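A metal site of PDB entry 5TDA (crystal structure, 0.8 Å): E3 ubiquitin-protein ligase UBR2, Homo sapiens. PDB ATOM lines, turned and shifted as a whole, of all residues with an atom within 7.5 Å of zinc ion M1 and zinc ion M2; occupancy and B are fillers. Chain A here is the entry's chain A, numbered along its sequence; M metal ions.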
ATOM      1  N   SER A   5      19.858  -1.749  -8.716  1.00  0.00           N
ATOM      2  CA  SER A   5      20.861  -1.265  -9.649  1.00  0.00           C
ATOM      3  C   SER A   5      21.310   0.145  -9.302  1.00  0.00           C
ATOM      4  O   SER A   5      22.395   0.560  -9.686  1.00  0.00           O
ATOM      5  CB  SER A   5      20.325  -1.338 -11.086  1.00  0.00           C
ATOM      6  N   LEU A   6      20.467   0.880  -8.572  1.00  0.00           N
ATOM      7  CA  LEU A   6      20.794   2.202  -8.046  1.00  0.00           C
ATOM      8  C   LEU A   6      21.007   2.102  -6.535  1.00  0.00           C
ATOM      9  O   LEU A   6      20.800   1.039  -5.933  1.00  0.00           O
ATOM     10  CB  LEU A   6      19.691   3.210  -8.375  1.00  0.00           C
ATOM     11  CG  LEU A   6      19.479   3.531  -9.863  1.00  0.00           C
ATOM     12  CD1 LEU A   6      18.401   4.592 -10.013  1.00  0.00           C
ATOM     13  CD2 LEU A   6      20.764   3.999 -10.526  1.00  0.00           C
ATOM     14  N   CYS A   7      21.444   3.204  -5.927  1.00  0.00           N
ATOM     15  CA  CYS A   7      21.836   3.172  -4.522  1.00  0.00           C
ATOM     16  C   CYS A   7      20.617   3.170  -3.590  1.00  0.00           C
ATOM     17  O   CYS A   7      20.269   2.137  -3.006  1.00  0.00           O
ATOM     18  CB  CYS A   7      22.775   4.347  -4.191  1.00  0.00           C
ATOM     19  SG  CYS A   7      23.321   4.260  -2.454  1.00  0.00           S
ATOM     20  N   GLY A   8      19.986   4.321  -3.430  1.00  0.00           N
ATOM     21  CA  GLY A   8      18.829   4.432  -2.548  1.00  0.00           C
ATOM     22  C   GLY A   8      19.099   4.282  -1.060  1.00  0.00           C
ATOM     23  O   GLY A   8      18.157   4.096  -0.283  1.00  0.00           O
ATOM     24  N   ARG A   9      20.359   4.359  -0.628  1.00  0.00           N
ATOM     25  CA  ARG A   9      20.682   4.190   0.784  1.00  0.00           C
ATOM     26  C   ARG A   9      20.014   5.279   1.611  1.00  0.00           C
ATOM     27  O   ARG A   9      20.050   6.463   1.277  1.00  0.00           O
ATOM     28  CB  ARG A   9      22.214   4.180   0.994  1.00  0.00           C
ATOM     29  CG  ARG A   9      22.854   2.786   0.699  1.00  0.00           C
ATOM     30  CD  ARG A   9      24.391   2.745   0.635  1.00  0.00           C
ATOM     31  NE  ARG A   9      25.028   3.227   1.864  1.00  0.00           N
ATOM     32  CZ  ARG A   9      26.306   3.068   2.174  1.00  0.00           C
ATOM     33  NH1 ARG A   9      26.761   3.586   3.285  1.00  0.00           N
ATOM     34  NH2 ARG A   9      27.134   2.388   1.386  1.00  0.00           N
ATOM     35  N   PHE A  11      20.507   7.004   5.163  1.00  0.00           N
ATOM     36  CA  PHE A  11      21.645   7.106   6.061  1.00  0.00           C
ATOM     37  C   PHE A  11      21.305   6.596   7.456  1.00  0.00           C
ATOM     38  O   PHE A  11      20.218   6.864   8.002  1.00  0.00           O
ATOM     39  CB  PHE A  11      22.125   8.557   6.175  1.00  0.00           C
ATOM     40  CG  PHE A  11      22.570   9.148   4.860  1.00  0.00           C
ATOM     41  CD1 PHE A  11      23.591   8.587   4.109  1.00  0.00           C
ATOM     42  CD2 PHE A  11      21.957  10.280   4.378  1.00  0.00           C
ATOM     43  CE1 PHE A  11      23.968   9.157   2.897  1.00  0.00           C
ATOM     44  CE2 PHE A  11      22.334  10.859   3.177  1.00  0.00           C
ATOM     45  CZ  PHE A  11      23.331  10.306   2.439  1.00  0.00           C
ATOM     46  N   GLU A  15      26.788   7.560  10.100  1.00  0.00           N
ATOM     47  CA  GLU A  15      27.316   7.224   8.791  1.00  0.00           C
ATOM     48  C   GLU A  15      27.965   8.446   8.146  1.00  0.00           C
ATOM     49  O   GLU A  15      27.357   9.518   8.123  1.00  0.00           O
ATOM     50  CB  GLU A  15      26.152   6.751   7.935  1.00  0.00           C
ATOM     51  CG  GLU A  15      26.598   6.267   6.595  1.00  0.00           C
ATOM     52  CD  GLU A  15      25.510   5.610   5.798  1.00  0.00           C
ATOM     53  OE1 GLU A  15      25.722   5.547   4.566  1.00  0.00           O
ATOM     54  OE2 GLU A  15      24.492   5.139   6.344  1.00  0.00           O
ATOM     55  N   VAL A  30      23.587  15.121  -1.447  1.00  0.00           N
ATOM     56  CA  VAL A  30      24.605  14.388  -0.701  1.00  0.00           C
ATOM     57  C   VAL A  30      24.742  12.972  -1.263  1.00  0.00           C
ATOM     58  O   VAL A  30      23.851  12.456  -1.946  1.00  0.00           O
ATOM     59  CB  VAL A  30      24.278  14.306   0.818  1.00  0.00           C
ATOM     60  CG1 VAL A  30      24.611  15.616   1.505  1.00  0.00           C
ATOM     61  CG2 VAL A  30      22.824  13.880   1.048  1.00  0.00           C
ATOM     62  N   LEU A  31      25.880  12.359  -0.941  1.00  0.00           N
ATOM     63  CA  LEU A  31      26.226  10.996  -1.332  1.00  0.00           C
ATOM     64  C   LEU A  31      26.694  10.211  -0.093  1.00  0.00           C
ATOM     65  O   LEU A  31      27.340  10.754   0.800  1.00  0.00           O
ATOM     66  CB  LEU A  31      27.382  10.989  -2.351  1.00  0.00           C
ATOM     67  CG  LEU A  31      27.079  11.685  -3.679  1.00  0.00           C
ATOM     68  CD1 LEU A  31      28.331  11.846  -4.525  1.00  0.00           C
ATOM     69  CD2 LEU A  31      26.000  10.949  -4.463  1.00  0.00           C
ATOM     70  N   CYS A  32      26.364   8.928  -0.089  1.00  0.00           N
ATOM     71  CA  CYS A  32      26.975   8.003   0.850  1.00  0.00           C
ATOM     72  C   CYS A  32      28.459   7.835   0.511  1.00  0.00           C
ATOM     73  O   CYS A  32      28.930   8.235  -0.551  1.00  0.00           O
ATOM     74  CB  CYS A  32      26.231   6.661   0.864  1.00  0.00           C
ATOM     75  SG  CYS A  32      26.530   5.604  -0.605  1.00  0.00           S
ATOM     76  N   MET A  33      29.205   7.198   1.425  1.00  0.00           N
ATOM     77  CA  MET A  33      30.642   7.070   1.229  1.00  0.00           C
ATOM     78  C   MET A  33      30.972   6.192   0.027  1.00  0.00           C
ATOM     79  O   MET A  33      31.928   6.475  -0.712  1.00  0.00           O
ATOM     80  CB  MET A  33      31.250   6.498   2.508  1.00  0.00           C
ATOM     81  CG  MET A  33      32.714   6.697   2.600  1.00  0.00           C
ATOM     82  SD  MET A  33      33.232   6.340   4.272  1.00  0.00           S
ATOM     83  CE  MET A  33      35.007   6.543   4.072  1.00  0.00           C
ATOM     84  N   GLU A  34      30.223   5.090  -0.151  1.00  0.00           N
ATOM     85  CA  GLU A  34      30.436   4.202  -1.289  1.00  0.00           C
ATOM     86  C   GLU A  34      30.320   4.980  -2.603  1.00  0.00           C
ATOM     87  O   GLU A  34      31.163   4.855  -3.512  1.00  0.00           O
ATOM     88  CB  GLU A  34      29.384   3.082  -1.246  1.00  0.00           C
ATOM     89  CG  GLU A  34      29.399   2.145  -2.456  1.00  0.00           C
ATOM     90  CD  GLU A  34      28.313   1.070  -2.425  1.00  0.00           C
ATOM     91  OE1 GLU A  34      27.373   1.164  -1.593  1.00  0.00           O
ATOM     92  OE2 GLU A  34      28.397   0.121  -3.238  1.00  0.00           O
ATOM     93  N   CYS A  35      29.277   5.789  -2.720  1.00  0.00           N
ATOM     94  CA  CYS A  35      29.048   6.513  -3.968  1.00  0.00           C
ATOM     95  C   CYS A  35      30.012   7.679  -4.128  1.00  0.00           C
ATOM     96  O   CYS A  35      30.533   7.916  -5.225  1.00  0.00           O
ATOM     97  CB  CYS A  35      27.580   6.952  -4.037  1.00  0.00           C
ATOM     98  SG  CYS A  35      26.467   5.503  -4.092  1.00  0.00           S
ATOM     99  N   PHE A  36      30.297   8.408  -3.034  1.00  0.00           N
ATOM    100  CA  PHE A  36      31.250   9.517  -3.134  1.00  0.00           C
ATOM    101  C   PHE A  36      32.614   9.027  -3.623  1.00  0.00           C
ATOM    102  O   PHE A  36      33.177   9.573  -4.588  1.00  0.00           O
ATOM    103  CB  PHE A  36      31.385  10.222  -1.776  1.00  0.00           C
ATOM    104  CG  PHE A  36      32.402  11.331  -1.799  1.00  0.00           C
ATOM    105  CD1 PHE A  36      32.124  12.518  -2.458  1.00  0.00           C
ATOM    106  CD2 PHE A  36      33.648  11.169  -1.214  1.00  0.00           C
ATOM    107  CE1 PHE A  36      33.060  13.541  -2.511  1.00  0.00           C
ATOM    108  CE2 PHE A  36      34.602  12.185  -1.260  1.00  0.00           C
ATOM    109  CZ  PHE A  36      34.303  13.379  -1.916  1.00  0.00           C
ATOM    110  N   GLY A  38      33.441   6.349  -5.142  1.00  0.00           N
ATOM    111  CA  GLY A  38      33.363   5.758  -6.469  1.00  0.00           C
ATOM    112  C   GLY A  38      32.974   6.732  -7.561  1.00  0.00           C
ATOM    113  O   GLY A  38      32.743   6.298  -8.698  1.00  0.00           O
ATOM    114  N   SER A  39      32.928   8.032  -7.254  1.00  0.00           N
ATOM    115  CA  SER A  39      32.504   9.061  -8.189  1.00  0.00           C
ATOM    116  C   SER A  39      33.662   9.999  -8.513  1.00  0.00           C
ATOM    117  O   SER A  39      34.711  10.000  -7.828  1.00  0.00           O
ATOM    118  CB  SER A  39      31.353   9.900  -7.590  1.00  0.00           C
ATOM    119  OG  SER A  39      31.829  10.838  -6.640  1.00  0.00           O
ATOM    120  N   PHE A  56      18.839  10.489   2.578  1.00  0.00           N
ATOM    121  CA  PHE A  56      19.185   9.458   1.604  1.00  0.00           C
ATOM    122  C   PHE A  56      20.274   9.928   0.637  1.00  0.00           C
ATOM    123  O   PHE A  56      20.458  11.125   0.378  1.00  0.00           O
ATOM    124  CB  PHE A  56      17.942   8.958   0.847  1.00  0.00           C
ATOM    125  CG  PHE A  56      17.208  10.052   0.088  1.00  0.00           C
ATOM    126  CD1 PHE A  56      16.199  10.798   0.695  1.00  0.00           C
ATOM    127  CD2 PHE A  56      17.513  10.300  -1.247  1.00  0.00           C
ATOM    128  CE1 PHE A  56      15.520  11.790  -0.013  1.00  0.00           C
ATOM    129  CE2 PHE A  56      16.819  11.277  -1.960  1.00  0.00           C
ATOM    130  CZ  PHE A  56      15.815  12.020  -1.340  1.00  0.00           C
ATOM    131  N   CYS A  57      20.953   8.930   0.070  1.00  0.00           N
ATOM    132  CA  CYS A  57      21.961   9.178  -0.948  1.00  0.00           C
ATOM    133  C   CYS A  57      21.311   9.600  -2.275  1.00  0.00           C
ATOM    134  O   CYS A  57      20.332   8.988  -2.725  1.00  0.00           O
ATOM    135  CB  CYS A  57      22.764   7.875  -1.153  1.00  0.00           C
ATOM    136  SG  CYS A  57      24.063   8.073  -2.407  1.00  0.00           S
ATOM    137  N   ASP A  58      21.881  10.635  -2.906  1.00  0.00           N
ATOM    138  CA  ASP A  58      21.380  11.187  -4.157  1.00  0.00           C
ATOM    139  C   ASP A  58      22.098  10.648  -5.399  1.00  0.00           C
ATOM    140  O   ASP A  58      21.954  11.214  -6.490  1.00  0.00           O
ATOM    141  CB  ASP A  58      21.443  12.719  -4.118  1.00  0.00           C
ATOM    142  CG  ASP A  58      20.575  13.307  -3.004  1.00  0.00           C
ATOM    143  OD1 ASP A  58      19.374  12.923  -2.959  1.00  0.00           O
ATOM    144  OD2 ASP A  58      21.082  14.103  -2.202  1.00  0.00           O
ATOM    145  N   CYS A  59      22.862   9.560  -5.256  1.00  0.00           N
ATOM    146  CA  CYS A  59      23.496   8.956  -6.433  1.00  0.00           C
ATOM    147  C   CYS A  59      22.406   8.549  -7.421  1.00  0.00           C
ATOM    148  O   CYS A  59      21.434   7.893  -7.051  1.00  0.00           O
ATOM    149  CB  CYS A  59      24.304   7.729  -5.998  1.00  0.00           C
ATOM    150  SG  CYS A  59      25.087   6.890  -7.410  1.00  0.00           S
ATOM    151  N   GLY A  60      22.592   8.927  -8.692  1.00  0.00           N
ATOM    152  CA  GLY A  60      21.651   8.592  -9.733  1.00  0.00           C
ATOM    153  C   GLY A  60      20.583   9.623 -10.007  1.00  0.00           C
ATOM    154  O   GLY A  60      19.897   9.517 -11.029  1.00  0.00           O
ATOM    155  N   PRO A  69      26.539  12.497 -12.074  1.00  0.00           N
ATOM    156  CA  PRO A  69      25.347  12.160 -11.271  1.00  0.00           C
ATOM    157  C   PRO A  69      25.334  10.756 -10.707  1.00  0.00           C
ATOM    158  O   PRO A  69      24.474  10.468  -9.859  1.00  0.00           O
ATOM    159  CB  PRO A  69      24.190  12.363 -12.249  1.00  0.00           C
ATOM    160  CG  PRO A  69      24.802  12.085 -13.571  1.00  0.00           C
ATOM    161  CD  PRO A  69      26.213  12.647 -13.498  1.00  0.00           C
ATOM    162  N   TYR A  70      26.228   9.873 -11.175  1.00  0.00           N
ATOM    163  CA  TYR A  70      26.334   8.489 -10.760  1.00  0.00           C
ATOM    164  C   TYR A  70      27.761   8.203 -10.280  1.00  0.00           C
ATOM    165  O   TYR A  70      28.712   8.932 -10.573  1.00  0.00           O
ATOM    166  CB  TYR A  70      26.013   7.515 -11.931  1.00  0.00           C
ATOM    167  CG  TYR A  70      24.564   7.489 -12.409  1.00  0.00           C
ATOM    168  CD1 TYR A  70      24.112   8.412 -13.355  1.00  0.00           C
ATOM    169  CD2 TYR A  70      23.671   6.537 -11.958  1.00  0.00           C
ATOM    170  CE1 TYR A  70      22.800   8.387 -13.805  1.00  0.00           C
ATOM    171  CE2 TYR A  70      22.365   6.500 -12.406  1.00  0.00           C
ATOM    172  CZ  TYR A  70      21.931   7.424 -13.335  1.00  0.00           C
ATOM    173  OH  TYR A  70      20.625   7.396 -13.772  1.00  0.00           O
ATOM    174  N   CYS A  71      27.905   7.132  -9.499  1.00  0.00           N
ATOM    175  CA  CYS A  71      29.203   6.552  -9.205  1.00  0.00           C
ATOM    176  C   CYS A  71      29.431   5.327 -10.094  1.00  0.00           C
ATOM    177  O   CYS A  71      28.548   4.891 -10.838  1.00  0.00           O
ATOM    178  CB  CYS A  71      29.293   6.159  -7.739  1.00  0.00           C
ATOM    179  SG  CYS A  71      28.339   4.659  -7.344  1.00  0.00           S
ATOM    180  N   GLN A  72      30.626   4.772  -9.964  1.00  0.00           N
ATOM    181  CA  GLN A  72      31.023   3.665 -10.814  1.00  0.00           C
ATOM    182  C   GLN A  72      30.173   2.414 -10.561  1.00  0.00           C
ATOM    183  O   GLN A  72      29.968   1.626 -11.498  1.00  0.00           O
ATOM    184  CB  GLN A  72      32.519   3.422 -10.606  1.00  0.00           C
ATOM    185  CG  GLN A  72      33.143   2.495 -11.575  1.00  0.00           C
ATOM    186  CD  GLN A  72      33.064   1.082 -11.088  1.00  0.00           C
ATOM    187  OE1 GLN A  72      32.767   0.833  -9.932  1.00  0.00           O
ATOM    188  NE2 GLN A  72      33.386   0.132 -11.965  1.00  0.00           N
ATOM    189  N   LYS A  73      29.654   2.213  -9.335  1.00  0.00           N
ATOM    190  CA  LYS A  73      28.808   1.050  -9.027  1.00  0.00           C
ATOM    191  C   LYS A  73      27.414   1.151  -9.644  1.00  0.00           C
ATOM    192  O   LYS A  73      26.806   0.126  -9.973  1.00  0.00           O
ATOM    193  CB  LYS A  73      28.624   0.905  -7.499  1.00  0.00           C
ATOM    194  CG  LYS A  73      29.811   0.338  -6.756  1.00  0.00           C
ATOM    195  CD  LYS A  73      30.012  -1.139  -7.029  1.00  0.00           C
ATOM    196  CE  LYS A  73      30.633  -1.847  -5.810  1.00  0.00           C
ATOM    197  NZ  LYS A  73      29.664  -2.069  -4.682  1.00  0.00           N
ATOM    198  N   HIS A  74      26.867   2.351  -9.762  1.00  0.00           N
ATOM    199  CA  HIS A  74      25.452   2.518 -10.090  1.00  0.00           C
ATOM    200  C   HIS A  74      25.210   3.042 -11.492  1.00  0.00           C
ATOM    201  O   HIS A  74      24.045   3.132 -11.910  1.00  0.00           O
ATOM    202  CB  HIS A  74      24.745   3.354  -9.023  1.00  0.00           C
ATOM    203  CG  HIS A  74      24.825   2.722  -7.668  1.00  0.00           C
ATOM    204  ND1 HIS A  74      25.423   3.321  -6.580  1.00  0.00           N
ATOM    205  CD2 HIS A  74      24.463   1.475  -7.282  1.00  0.00           C
ATOM    206  CE1 HIS A  74      25.387   2.465  -5.565  1.00  0.00           C
ATOM    207  NE2 HIS A  74      24.809   1.342  -5.958  1.00  0.00           N
ATOM    208  N   GLU A  75      26.289   3.305 -12.251  1.00  0.00           N
ATOM    209  CA  GLU A  75      26.160   3.806 -13.613  1.00  0.00           C
ATOM    210  C   GLU A  75      25.616   2.732 -14.557  1.00  0.00           C
ATOM    211  O   GLU A  75      25.178   3.052 -15.669  1.00  0.00           O
ATOM    212  CB  GLU A  75      27.512   4.294 -14.124  1.00  0.00           C
ATOM    213  CG  GLU A  75      28.613   3.257 -14.136  1.00  0.00           C
ATOM    214  CD  GLU A  75      29.943   3.845 -14.538  1.00  0.00           C
ATOM    215  OE1 GLU A  75      29.927   4.950 -15.103  1.00  0.00           O
ATOM    216  OE2 GLU A  75      30.987   3.221 -14.282  1.00  0.00           O
HETATM  217 ZN    ZN M   1      24.945   5.912  -2.300  1.00  0.00          ZN
HETATM  218 ZN    ZN M   2      26.270   5.179  -6.406  1.00  0.00          ZN
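The backbone carbonyl oxygen of Arg 9 lies within hydrogen-bond range of the backbone NH of Cys 57 (2.9 Å).
SG of Cys 32 lies close to N of Glu 34.
SG of Cys 7 sits close to N of Arg 9, at 3.5 Å.
N of Lys 73 lies close to SG of Cys 71 (3.4 Å).
The backbone carbonyl oxygen of Cys 35 sits close to the side-chain hydroxyl of Ser 39 (3.5 Å).
The side-chain sulfur (SG) of Cys 57 lies close to the backbone NH (N) of Cys 59 (3.4 Å).
The side-chain sulfur (SG) of Cys 32 lies close to the guanidinium group (NE) of Arg 9 (3.7 Å).
Of the 28 residues printed, 4 come within 4 Å of zinc ion M1.
Four residues have an atom within 4 Å of zinc ion M2: Cys 35, Cys 59, Cys 71 and His 74.
The nearest printed residue that does not touch zinc ion M2 is Cys 7 (4.2 Å).
Zinc ion M1 is bound by SG of Cys 7 (2.3 Å), SG of Cys 57 (2.3 Å), SG of Cys 32 (2.3 Å) and SG of Cys 35 (2.4 Å).
Zinc ion M1 has four donor atoms within binding distance.
Zinc ion M2 is bound by ND1 of His 74, SG of Cys 59, SG of Cys 71 and SG of Cys 35.
Zinc ion M2 has four donor atoms within binding distance.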
